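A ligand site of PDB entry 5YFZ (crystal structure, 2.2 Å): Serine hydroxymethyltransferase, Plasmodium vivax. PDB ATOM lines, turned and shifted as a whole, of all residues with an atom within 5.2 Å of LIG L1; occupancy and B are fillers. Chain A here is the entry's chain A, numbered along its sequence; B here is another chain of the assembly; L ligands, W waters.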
ATOM      1  N   ILE A  32     -16.849 -24.005 -30.801  1.00  0.00           N
ATOM      2  CA  ILE A  32     -17.440 -22.764 -30.269  1.00  0.00           C
ATOM      3  C   ILE A  32     -17.618 -22.925 -28.764  1.00  0.00           C
ATOM      4  O   ILE A  32     -18.189 -23.897 -28.327  1.00  0.00           O
ATOM      5  CB  ILE A  32     -18.761 -22.372 -30.952  1.00  0.00           C
ATOM      6  CG1 ILE A  32     -18.578 -22.247 -32.481  1.00  0.00           C
ATOM      7  CG2 ILE A  32     -19.289 -21.054 -30.384  1.00  0.00           C
ATOM      8  CD1 ILE A  32     -17.715 -21.062 -32.927  1.00  0.00           C
ATOM      9  N   SER A  34     -19.271 -21.468 -26.563  1.00  0.00           N
ATOM     10  CA  SER A  34     -20.703 -21.390 -26.159  1.00  0.00           C
ATOM     11  C   SER A  34     -21.680 -22.378 -26.757  1.00  0.00           C
ATOM     12  O   SER A  34     -22.847 -22.312 -26.432  1.00  0.00           O
ATOM     13  CB  SER A  34     -21.226 -19.959 -26.365  1.00  0.00           C
ATOM     14  OG  SER A  34     -20.787 -19.352 -27.557  1.00  0.00           O
ATOM     15  N   SER A 100     -33.833 -15.941 -22.691  1.00  0.00           N
ATOM     16  CA  SER A 100     -32.447 -16.211 -23.058  1.00  0.00           C
ATOM     17  C   SER A 100     -31.522 -15.460 -22.121  1.00  0.00           C
ATOM     18  O   SER A 100     -31.977 -14.671 -21.333  1.00  0.00           O
ATOM     19  CB  SER A 100     -32.180 -15.768 -24.515  1.00  0.00           C
ATOM     20  OG  SER A 100     -31.270 -16.664 -25.162  1.00  0.00           O
ATOM     21  N   GLY A 101     -30.227 -15.687 -22.243  1.00  0.00           N
ATOM     22  CA  GLY A 101     -29.246 -15.091 -21.358  1.00  0.00           C
ATOM     23  C   GLY A 101     -29.258 -13.577 -21.234  1.00  0.00           C
ATOM     24  O   GLY A 101     -29.140 -13.051 -20.133  1.00  0.00           O
ATOM     25  N   SER A 102     -29.361 -12.870 -22.364  1.00  0.00           N
ATOM     26  CA  SER A 102     -29.318 -11.409 -22.352  1.00  0.00           C
ATOM     27  C   SER A 102     -30.548 -10.821 -21.627  1.00  0.00           C
ATOM     28  O   SER A 102     -30.449  -9.889 -20.855  1.00  0.00           O
ATOM     29  CB  SER A 102     -29.204 -10.851 -23.789  1.00  0.00           C
ATOM     30  OG  SER A 102     -28.229 -11.521 -24.601  1.00  0.00           O
ATOM     31  N   ALA A 103     -31.712 -11.369 -21.930  1.00  0.00           N
ATOM     32  CA  ALA A 103     -32.956 -11.040 -21.218  1.00  0.00           C
ATOM     33  C   ALA A 103     -32.800 -11.258 -19.692  1.00  0.00           C
ATOM     34  O   ALA A 103     -33.032 -10.357 -18.914  1.00  0.00           O
ATOM     35  CB  ALA A 103     -34.102 -11.874 -21.763  1.00  0.00           C
ATOM     36  N   ASN A 105     -30.160 -11.337 -17.878  1.00  0.00           N
ATOM     37  CA  ASN A 105     -29.259 -10.331 -17.315  1.00  0.00           C
ATOM     38  C   ASN A 105     -29.880  -8.937 -17.209  1.00  0.00           C
ATOM     39  O   ASN A 105     -29.738  -8.283 -16.171  1.00  0.00           O
ATOM     40  CB  ASN A 105     -27.955 -10.223 -18.119  1.00  0.00           C
ATOM     41  CG  ASN A 105     -26.952 -11.340 -17.809  1.00  0.00           C
ATOM     42  OD1 ASN A 105     -27.176 -12.228 -16.972  1.00  0.00           O
ATOM     43  ND2 ASN A 105     -25.811 -11.273 -18.494  1.00  0.00           N
ATOM     44  N   HIS A 129     -19.365  -9.841 -21.250  1.00  0.00           N
ATOM     45  CA  HIS A 129     -20.498  -9.917 -22.151  1.00  0.00           C
ATOM     46  C   HIS A 129     -21.060  -8.544 -22.427  1.00  0.00           C
ATOM     47  O   HIS A 129     -20.870  -7.617 -21.655  1.00  0.00           O
ATOM     48  CB  HIS A 129     -21.615 -10.797 -21.588  1.00  0.00           C
ATOM     49  CG  HIS A 129     -22.622 -11.220 -22.617  1.00  0.00           C
ATOM     50  ND1 HIS A 129     -23.934 -10.819 -22.579  1.00  0.00           N
ATOM     51  CD2 HIS A 129     -22.486 -11.981 -23.736  1.00  0.00           C
ATOM     52  CE1 HIS A 129     -24.576 -11.311 -23.626  1.00  0.00           C
ATOM     53  NE2 HIS A 129     -23.728 -12.041 -24.324  1.00  0.00           N
ATOM     54  N   THR A 131     -24.095  -7.576 -22.250  1.00  0.00           N
ATOM     55  CA  THR A 131     -25.031  -7.217 -21.187  1.00  0.00           C
ATOM     56  C   THR A 131     -24.395  -6.933 -19.826  1.00  0.00           C
ATOM     57  O   THR A 131     -25.105  -6.804 -18.833  1.00  0.00           O
ATOM     58  CB  THR A 131     -26.059  -8.342 -20.965  1.00  0.00           C
ATOM     59  OG1 THR A 131     -25.380  -9.565 -20.656  1.00  0.00           O
ATOM     60  CG2 THR A 131     -26.914  -8.516 -22.173  1.00  0.00           C
ATOM     61  N   HIS A 132     -23.057  -6.822 -19.757  1.00  0.00           N
ATOM     62  CA  HIS A 132     -22.383  -6.406 -18.533  1.00  0.00           C
ATOM     63  C   HIS A 132     -22.069  -4.919 -18.567  1.00  0.00           C
ATOM     64  O   HIS A 132     -21.259  -4.446 -17.792  1.00  0.00           O
ATOM     65  CB  HIS A 132     -21.131  -7.269 -18.281  1.00  0.00           C
ATOM     66  CG  HIS A 132     -21.434  -8.735 -18.129  1.00  0.00           C
ATOM     67  ND1 HIS A 132     -20.458  -9.704 -18.101  1.00  0.00           N
ATOM     68  CD2 HIS A 132     -22.619  -9.387 -18.016  1.00  0.00           C
ATOM     69  CE1 HIS A 132     -21.028 -10.900 -17.978  1.00  0.00           C
ATOM     70  NE2 HIS A 132     -22.340 -10.724 -17.929  1.00  0.00           N
ATOM     71  N   GLY A 181     -18.125 -13.091 -13.776  1.00  0.00           N
ATOM     72  CA  GLY A 181     -18.489 -14.223 -14.653  1.00  0.00           C
ATOM     73  C   GLY A 181     -18.532 -13.684 -16.066  1.00  0.00           C
ATOM     74  O   GLY A 181     -19.082 -12.584 -16.302  1.00  0.00           O
ATOM     75  N   TYR A 182     -17.937 -14.405 -17.020  1.00  0.00           N
ATOM     76  CA  TYR A 182     -17.565 -13.797 -18.324  1.00  0.00           C
ATOM     77  C   TYR A 182     -17.794 -14.686 -19.541  1.00  0.00           C
ATOM     78  O   TYR A 182     -18.183 -15.832 -19.418  1.00  0.00           O
ATOM     79  CB  TYR A 182     -16.124 -13.334 -18.260  1.00  0.00           C
ATOM     80  CG  TYR A 182     -15.743 -12.662 -16.951  1.00  0.00           C
ATOM     81  CD1 TYR A 182     -16.074 -11.327 -16.712  1.00  0.00           C
ATOM     82  CD2 TYR A 182     -15.066 -13.364 -15.956  1.00  0.00           C
ATOM     83  CE1 TYR A 182     -15.728 -10.703 -15.527  1.00  0.00           C
ATOM     84  CE2 TYR A 182     -14.721 -12.750 -14.769  1.00  0.00           C
ATOM     85  CZ  TYR A 182     -15.053 -11.420 -14.559  1.00  0.00           C
ATOM     86  OH  TYR A 182     -14.720 -10.814 -13.371  1.00  0.00           O
ATOM     87  N   THR A 183     -17.557 -14.136 -20.733  1.00  0.00           N
ATOM     88  CA  THR A 183     -17.851 -14.872 -21.969  1.00  0.00           C
ATOM     89  C   THR A 183     -16.617 -15.585 -22.538  1.00  0.00           C
ATOM     90  O   THR A 183     -16.725 -16.692 -23.033  1.00  0.00           O
ATOM     91  CB  THR A 183     -18.588 -14.064 -23.065  1.00  0.00           C
ATOM     92  OG1 THR A 183     -17.777 -13.947 -24.248  1.00  0.00           O
ATOM     93  CG2 THR A 183     -19.000 -12.746 -22.609  1.00  0.00           C
ATOM     94  N   ASP A 208     -22.531 -13.873 -13.402  1.00  0.00           N
ATOM     95  CA  ASP A 208     -23.063 -14.521 -14.623  1.00  0.00           C
ATOM     96  C   ASP A 208     -22.159 -15.677 -14.947  1.00  0.00           C
ATOM     97  O   ASP A 208     -21.087 -15.456 -15.488  1.00  0.00           O
ATOM     98  CB  ASP A 208     -23.088 -13.549 -15.802  1.00  0.00           C
ATOM     99  CG  ASP A 208     -23.702 -14.150 -17.073  1.00  0.00           C
ATOM    100  OD1 ASP A 208     -23.864 -15.390 -17.227  1.00  0.00           O
ATOM    101  OD2 ASP A 208     -24.026 -13.323 -17.939  1.00  0.00           O
ATOM    102  N   SER A 210     -22.888 -18.404 -17.030  1.00  0.00           N
ATOM    103  CA  SER A 210     -23.341 -19.069 -18.259  1.00  0.00           C
ATOM    104  C   SER A 210     -22.350 -20.028 -18.945  1.00  0.00           C
ATOM    105  O   SER A 210     -22.751 -21.114 -19.392  1.00  0.00           O
ATOM    106  CB  SER A 210     -23.769 -17.987 -19.244  1.00  0.00           C
ATOM    107  OG  SER A 210     -25.002 -17.416 -18.831  1.00  0.00           O
ATOM    108  N   HIS A 211     -21.096 -19.620 -19.073  1.00  0.00           N
ATOM    109  CA  HIS A 211     -20.056 -20.464 -19.700  1.00  0.00           C
ATOM    110  C   HIS A 211     -19.480 -21.594 -18.827  1.00  0.00           C
ATOM    111  O   HIS A 211     -18.889 -22.547 -19.372  1.00  0.00           O
ATOM    112  CB  HIS A 211     -18.888 -19.630 -20.182  1.00  0.00           C
ATOM    113  CG  HIS A 211     -19.066 -19.100 -21.553  1.00  0.00           C
ATOM    114  ND1 HIS A 211     -18.764 -19.840 -22.676  1.00  0.00           N
ATOM    115  CD2 HIS A 211     -19.491 -17.905 -21.990  1.00  0.00           C
ATOM    116  CE1 HIS A 211     -18.997 -19.110 -23.749  1.00  0.00           C
ATOM    117  NE2 HIS A 211     -19.442 -17.934 -23.368  1.00  0.00           N
ATOM    118  N   THR A 234     -27.304 -19.119 -18.521  1.00  0.00           N
ATOM    119  CA  THR A 234     -27.952 -19.723 -19.669  1.00  0.00           C
ATOM    120  C   THR A 234     -27.978 -21.224 -19.489  1.00  0.00           C
ATOM    121  O   THR A 234     -27.108 -21.760 -18.851  1.00  0.00           O
ATOM    122  CB  THR A 234     -27.188 -19.371 -20.966  1.00  0.00           C
ATOM    123  OG1 THR A 234     -25.800 -19.711 -20.822  1.00  0.00           O
ATOM    124  CG2 THR A 234     -27.318 -17.914 -21.259  1.00  0.00           C
ATOM    125  N   HIS A 236     -27.968 -23.398 -22.257  1.00  0.00           N
ATOM    126  CA  HIS A 236     -27.664 -23.996 -23.610  1.00  0.00           C
ATOM    127  C   HIS A 236     -26.201 -24.230 -23.934  1.00  0.00           C
ATOM    128  O   HIS A 236     -25.892 -24.905 -24.917  1.00  0.00           O
ATOM    129  CB  HIS A 236     -28.268 -23.197 -24.787  1.00  0.00           C
ATOM    130  CG  HIS A 236     -28.153 -21.714 -24.647  1.00  0.00           C
ATOM    131  ND1 HIS A 236     -28.966 -20.987 -23.816  1.00  0.00           N
ATOM    132  CD2 HIS A 236     -27.374 -20.808 -25.285  1.00  0.00           C
ATOM    133  CE1 HIS A 236     -28.686 -19.704 -23.924  1.00  0.00           C
ATOM    134  NE2 HIS A 236     -27.710 -19.571 -24.804  1.00  0.00           N
ATOM    135  N   LYS A 237     -25.296 -23.677 -23.133  1.00  0.00           N
ATOM    136  CA  LYS A 237     -23.883 -23.883 -23.360  1.00  0.00           C
ATOM    137  C   LYS A 237     -23.448 -25.215 -22.704  1.00  0.00           C
ATOM    138  O   LYS A 237     -24.006 -26.305 -22.998  1.00  0.00           O
ATOM    139  CB  LYS A 237     -23.116 -22.670 -22.865  1.00  0.00           C
ATOM    140  CG  LYS A 237     -23.567 -21.357 -23.467  1.00  0.00           C
ATOM    141  CD  LYS A 237     -22.806 -20.211 -22.847  1.00  0.00           C
ATOM    142  CE  LYS A 237     -23.205 -18.899 -23.459  1.00  0.00           C
ATOM    143  NZ  LYS A 237     -24.658 -18.702 -23.322  1.00  0.00           N
ATOM    144  N   ARG A 243     -32.181 -23.420 -25.311  1.00  0.00           N
ATOM    145  CA  ARG A 243     -31.867 -22.025 -25.227  1.00  0.00           C
ATOM    146  C   ARG A 243     -32.850 -21.377 -24.269  1.00  0.00           C
ATOM    147  O   ARG A 243     -33.993 -21.179 -24.600  1.00  0.00           O
ATOM    148  CB  ARG A 243     -31.896 -21.347 -26.605  1.00  0.00           C
ATOM    149  CG  ARG A 243     -30.964 -22.005 -27.612  1.00  0.00           C
ATOM    150  CD  ARG A 243     -30.874 -21.211 -28.910  1.00  0.00           C
ATOM    151  NE  ARG A 243     -29.841 -20.182 -28.870  1.00  0.00           N
ATOM    152  CZ  ARG A 243     -28.557 -20.372 -29.079  1.00  0.00           C
ATOM    153  NH1 ARG A 243     -28.060 -21.575 -29.333  1.00  0.00           N
ATOM    154  NH2 ARG A 243     -27.747 -19.333 -28.979  1.00  0.00           N
ATOM    155  N   ARG A 371     -11.128 -17.858 -30.053  1.00  0.00           N
ATOM    156  CA  ARG A 371     -11.538 -18.585 -28.869  1.00  0.00           C
ATOM    157  C   ARG A 371     -12.018 -19.949 -29.285  1.00  0.00           C
ATOM    158  O   ARG A 371     -12.782 -20.073 -30.248  1.00  0.00           O
ATOM    159  CB  ARG A 371     -12.654 -17.814 -28.158  1.00  0.00           C
ATOM    160  CG  ARG A 371     -13.171 -18.444 -26.890  1.00  0.00           C
ATOM    161  CD  ARG A 371     -14.433 -17.730 -26.402  1.00  0.00           C
ATOM    162  NE  ARG A 371     -15.587 -18.144 -27.198  1.00  0.00           N
ATOM    163  CZ  ARG A 371     -16.849 -17.774 -27.002  1.00  0.00           C
ATOM    164  NH1 ARG A 371     -17.199 -16.982 -25.980  1.00  0.00           N
ATOM    165  NH2 ARG A 371     -17.789 -18.245 -27.838  1.00  0.00           N
ATOM    166  N   TYR B  54     -25.144 -20.938 -32.812  1.00  0.00           N
ATOM    167  CA  TYR B  54     -25.013 -19.583 -32.292  1.00  0.00           C
ATOM    168  C   TYR B  54     -24.777 -18.698 -33.516  1.00  0.00           C
ATOM    169  O   TYR B  54     -23.789 -18.866 -34.228  1.00  0.00           O
ATOM    170  CB  TYR B  54     -23.852 -19.440 -31.282  1.00  0.00           C
ATOM    171  CG  TYR B  54     -24.285 -18.885 -29.951  1.00  0.00           C
ATOM    172  CD1 TYR B  54     -24.740 -17.582 -29.839  1.00  0.00           C
ATOM    173  CD2 TYR B  54     -24.279 -19.680 -28.785  1.00  0.00           C
ATOM    174  CE1 TYR B  54     -25.189 -17.087 -28.629  1.00  0.00           C
ATOM    175  CE2 TYR B  54     -24.707 -19.178 -27.566  1.00  0.00           C
ATOM    176  CZ  TYR B  54     -25.164 -17.892 -27.491  1.00  0.00           C
ATOM    177  OH  TYR B  54     -25.612 -17.389 -26.293  1.00  0.00           O
ATOM    178  N   GLU B  56     -25.193 -14.940 -33.832  1.00  0.00           N
ATOM    179  CA  GLU B  56     -25.342 -13.531 -33.465  1.00  0.00           C
ATOM    180  C   GLU B  56     -25.141 -12.599 -34.636  1.00  0.00           C
ATOM    181  O   GLU B  56     -24.283 -12.840 -35.477  1.00  0.00           O
ATOM    182  CB  GLU B  56     -24.360 -13.173 -32.363  1.00  0.00           C
ATOM    183  CG  GLU B  56     -24.647 -13.808 -31.013  1.00  0.00           C
ATOM    184  CD  GLU B  56     -23.626 -13.418 -29.978  1.00  0.00           C
ATOM    185  OE1 GLU B  56     -22.505 -13.981 -30.016  1.00  0.00           O
ATOM    186  OE2 GLU B  56     -23.903 -12.530 -29.147  1.00  0.00           O
ATOM    187  N   TYR B  64     -19.676 -15.061 -36.734  1.00  0.00           N
ATOM    188  CA  TYR B  64     -18.955 -16.285 -37.106  1.00  0.00           C
ATOM    189  C   TYR B  64     -19.336 -16.793 -38.476  1.00  0.00           C
ATOM    190  O   TYR B  64     -20.345 -16.394 -39.038  1.00  0.00           O
ATOM    191  CB  TYR B  64     -19.200 -17.440 -36.116  1.00  0.00           C
ATOM    192  CG  TYR B  64     -19.587 -17.077 -34.719  1.00  0.00           C
ATOM    193  CD1 TYR B  64     -18.881 -16.109 -33.995  1.00  0.00           C
ATOM    194  CD2 TYR B  64     -20.629 -17.739 -34.076  1.00  0.00           C
ATOM    195  CE1 TYR B  64     -19.225 -15.802 -32.689  1.00  0.00           C
ATOM    196  CE2 TYR B  64     -20.982 -17.432 -32.780  1.00  0.00           C
ATOM    197  CZ  TYR B  64     -20.276 -16.467 -32.076  1.00  0.00           C
ATOM    198  OH  TYR B  64     -20.643 -16.178 -30.776  1.00  0.00           O
ATOM    199  N   GLN B 270     -31.042  -8.273 -27.373  1.00  0.00           N
ATOM    200  CA  GLN B 270     -30.848  -9.719 -27.459  1.00  0.00           C
ATOM    201  C   GLN B 270     -29.393 -10.108 -27.733  1.00  0.00           C
ATOM    202  O   GLN B 270     -28.546  -9.274 -28.032  1.00  0.00           O
ATOM    203  CB  GLN B 270     -31.764 -10.332 -28.534  1.00  0.00           C
ATOM    204  CG  GLN B 270     -33.213  -9.836 -28.452  1.00  0.00           C
ATOM    205  CD  GLN B 270     -34.241 -10.767 -29.071  1.00  0.00           C
ATOM    206  OE1 GLN B 270     -35.347 -10.890 -28.538  1.00  0.00           O
ATOM    207  NE2 GLN B 270     -33.910 -11.400 -30.194  1.00  0.00           N
ATOM    208  N   GLY B 271     -29.128 -11.401 -27.593  1.00  0.00           N
ATOM    209  CA  GLY B 271     -27.880 -12.001 -27.981  1.00  0.00           C
ATOM    210  C   GLY B 271     -28.162 -12.895 -29.166  1.00  0.00           C
ATOM    211  O   GLY B 271     -28.635 -12.424 -30.200  1.00  0.00           O
ATOM    212  N   GLY B 272     -27.888 -14.196 -29.004  1.00  0.00           N
ATOM    213  CA  GLY B 272     -28.107 -15.171 -30.063  1.00  0.00           C
ATOM    214  C   GLY B 272     -29.580 -15.353 -30.424  1.00  0.00           C
ATOM    215  O   GLY B 272     -30.408 -15.448 -29.531  1.00  0.00           O
HETATM  216  N1  LIG L   1     -23.839 -14.052 -20.489  1.00  0.00           N
HETATM  217  C1  LIG L   1     -22.654 -14.549 -20.885  1.00  0.00           C
HETATM  218  C2  LIG L   1     -21.484 -14.594 -19.932  1.00  0.00           C
HETATM  219  C3  LIG L   1     -22.503 -15.042 -22.268  1.00  0.00           C
HETATM  220  O1  LIG L   1     -21.328 -15.548 -22.724  1.00  0.00           O
HETATM  221  C4  LIG L   1     -23.685 -14.992 -23.152  1.00  0.00           C
HETATM  222  C5  LIG L   1     -23.633 -15.475 -24.577  1.00  0.00           C
HETATM  223  C6  LIG L   1     -24.936 -14.433 -22.594  1.00  0.00           C
HETATM  224  C7  LIG L   1     -24.937 -13.969 -21.277  1.00  0.00           C
HETATM  225  C8  LIG L   1     -26.194 -14.286 -23.424  1.00  0.00           C
HETATM  226  O2  LIG L   1     -26.817 -15.488 -23.880  1.00  0.00           O
HETATM  227  P1  LIG L   1     -28.004 -15.273 -24.988  1.00  0.00           P
HETATM  228  O3  LIG L   1     -28.632 -13.909 -24.825  1.00  0.00           O
HETATM  229  O4  LIG L   1     -27.204 -15.348 -26.266  1.00  0.00           O
HETATM  230  O5  LIG L   1     -28.907 -16.418 -24.640  1.00  0.00           O
HETATM  231  C9  LIG L   1     -20.856 -16.391 -26.880  1.00  0.00           C
HETATM  232  O6  LIG L   1     -20.873 -16.703 -28.063  1.00  0.00           O
HETATM  233  O7  LIG L   1     -20.076 -16.960 -26.124  1.00  0.00           O
HETATM  234  C10 LIG L   1     -21.826 -15.341 -26.354  1.00  0.00           C
HETATM  235  N2  LIG L   1     -22.325 -15.805 -25.066  1.00  0.00           N
HETATM  236  C1  LG2 L   2     -17.612 -11.606 -28.582  1.00  0.00           C
HETATM  237  C2  LG2 L   2     -17.286 -13.104 -28.923  1.00  0.00           C
HETATM  238  C3  LG2 L   2     -19.045 -11.538 -28.177  1.00  0.00           C
HETATM  239  C4  LG2 L   2     -19.487 -11.485 -26.782  1.00  0.00           C
HETATM  240  C5  LG2 L   2     -15.473 -11.058 -27.659  1.00  0.00           C
HETATM  241  C6  LG2 L   2     -20.587 -11.579 -30.395  1.00  0.00           C
HETATM  242  C7  LG2 L   2     -17.918 -13.644 -30.215  1.00  0.00           C
HETATM  243  C8  LG2 L   2     -17.349 -10.605 -29.716  1.00  0.00           C
HETATM  244  C9  LG2 L   2     -18.029  -9.362 -29.866  1.00  0.00           C
HETATM  245  C10 LG2 L   2     -17.746  -8.468 -30.939  1.00  0.00           C
HETATM  246  C11 LG2 L   2     -16.078 -10.039 -31.695  1.00  0.00           C
HETATM  247  N1  LG2 L   2     -21.296 -11.470 -27.963  1.00  0.00           N
HETATM  248  C12 LG2 L   2     -17.165 -11.214 -26.112  1.00  0.00           C
HETATM  249  N2  LG2 L   2     -16.379 -10.946 -25.075  1.00  0.00           N
HETATM  250  C13 LG2 L   2     -16.705 -11.260 -27.396  1.00  0.00           C
HETATM  251  O1  LG2 L   2     -18.551 -11.470 -25.789  1.00  0.00           O
HETATM  252  C14 LG2 L   2     -20.332 -11.534 -28.909  1.00  0.00           C
HETATM  253  O2  LG2 L   2     -22.211  -4.066 -32.583  1.00  0.00           O
HETATM  254  C15 LG2 L   2     -21.316  -3.192 -32.564  1.00  0.00           C
HETATM  255  O3  LG2 L   2     -21.337  -2.181 -33.313  1.00  0.00           O
HETATM  256  C16 LG2 L   2     -20.134  -3.344 -31.621  1.00  0.00           C
HETATM  257  C17 LG2 L   2     -19.570  -4.765 -31.651  1.00  0.00           C
HETATM  258  C18 LG2 L   2     -18.099  -4.773 -31.315  1.00  0.00           C
HETATM  259  C19 LG2 L   2     -17.493  -6.125 -31.653  1.00  0.00           C
HETATM  260  C20 LG2 L   2     -20.294  -5.708 -30.711  1.00  0.00           C
HETATM  261  C21 LG2 L   2     -19.869  -7.152 -31.001  1.00  0.00           C
HETATM  262  N3  LG2 L   2     -18.393  -7.223 -31.161  1.00  0.00           N
HETATM  263  C22 LG2 L   2     -16.748  -8.848 -31.836  1.00  0.00           C
HETATM  264  F1  LG2 L   2     -15.128 -10.394 -32.555  1.00  0.00           F
HETATM  265  C23 LG2 L   2     -16.366 -10.910 -30.667  1.00  0.00           C
HETATM  266  C24 LG2 L   2     -17.533 -14.127 -27.785  1.00  0.00           C
HETATM  267  N4  LG2 L   2     -14.346 -10.872 -27.888  1.00  0.00           N
HETATM  268  N5  LG2 L   2     -20.824 -11.432 -26.638  1.00  0.00           N
HETATM  269  O   HOH W   1     -30.916 -13.734 -26.779  1.00  0.00           O
HETATM  270  O   HOH W   2     -24.891 -13.550 -26.727  1.00  0.00           O
HETATM  271  O   HOH W   3     -29.206 -17.782 -27.579  1.00  0.00           O
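Merely in contact with LIG L1: Asn 105, His 129, Tyr 182, Thr 183, Ser 210, Thr 234, Lys 237, Glu 56 of chain B and Gly 271 of chain B. Hydrophobic or aromatic side chains that line LIG L1: His 129, His 211, His 236 and Tyr 54 of chain B. Of the 27 residues printed, 20 come within 4 Å of LIG L1.
OD2 of Asp 208 lies within hydrogen-bond range of NE2 of His 132, 3.1 Å away. NE2 of His 236 lies within hydrogen-bond range of OH of Tyr 54 of chain B (3.4 Å). The side-chain amino group (NZ) of Lys 237 lies within hydrogen-bond range of the side-chain hydroxyl (OG1) of Thr 234. A ring nitrogen (ND1) of His 129 lies within hydrogen-bond range of the side-chain hydroxyl of Thr 131, at 2.7 Å. OG of Ser 34 sits at hydrogen-bond distance from NH2 of Arg 371. The backbone NH (N) of His 129 sits at hydrogen-bond distance from a ring nitrogen (ND1) of His 132 (3.3 Å). The side-chain hydroxyl (OG1) of Thr 131 lies within hydrogen-bond range of the side-chain amide nitrogen (ND2) of Asn 105. OD2 of Asp 208 is in hydrogen-bond range of ND2 of Asn 105, at 2.8 Å.
Water W2 lies within hydrogen-bond range of the side-chain carboxylate (OE2) of Glu 56 of chain B (2.8 Å), an oxygen (O4) of LIG L1 (3.0 Å) and a ring nitrogen (NE2) of His 129 (3.1 Å). Water W1 lies within hydrogen-bond range of O3 of LIG L1 (3.0 Å), N of Gly 271 of chain B (3.0 Å), O of Gly 272 of chain B (3.3 Å) and OG of Ser 100 (3.4 Å). Water W3 lies within hydrogen-bond range of the guanidinium group (NH2) of Arg 243 (2.5 Å), an oxygen (O5) of LIG L1 (3.3 Å), the backbone carbonyl oxygen (O) of Gly 272 of chain B (3.3 Å) and the side-chain hydroxyl (OG) of Ser 100 (3.4 Å).
N1 of LIG L1 sits at hydrogen-bond distance from OD2 of Asp 208 (2.7 Å). O5 of LIG L1 is in hydrogen-bond range of OG of Ser 100 (2.4 Å). The backbone NH (N) of Ser 102 sits at hydrogen-bond distance from an oxygen (O3) of LIG L1. An oxygen (O6) of LIG L1 is in hydrogen-bond range of the side-chain hydroxyl of Ser 34, at 2.7 Å. The side-chain hydroxyl (OG1) of Thr 183 sits at hydrogen-bond distance from an oxygen (O1) of LG2 L2, 3.0 Å away. The side-chain hydroxyl of Tyr 54 of chain B sits at hydrogen-bond distance from an oxygen (O4) of LIG L1 (2.6 Å). An oxygen (O4) of LIG L1 sits at hydrogen-bond distance from the backbone NH (N) of Gly 272 of chain B, at 3.0 Å. An oxygen (O7) of LIG L1 is in hydrogen-bond range of a ring nitrogen (NE2) of His 211, 3.0 Å away. OG of Ser 102 is in hydrogen-bond range of O3 of LIG L1 (2.4 Å). O7 of LIG L1 is in salt-bridge range of NH1 of Arg 371 (2.9 Å). An oxygen (O5) of LIG L1 sits at hydrogen-bond distance from the backbone NH (N) of Gly 101 (2.8 Å). An oxygen (O6) of LIG L1 lies within hydrogen-bond range of the side-chain hydroxyl of Tyr 64 of chain B. OE2 of Glu 56 of chain B lies within hydrogen-bond range of N1 of LG2 L2, 3.1 Å away. A ring nitrogen (NE2) of His 236 lies close to an oxygen (O5) of LIG L1 (3.4 Å).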
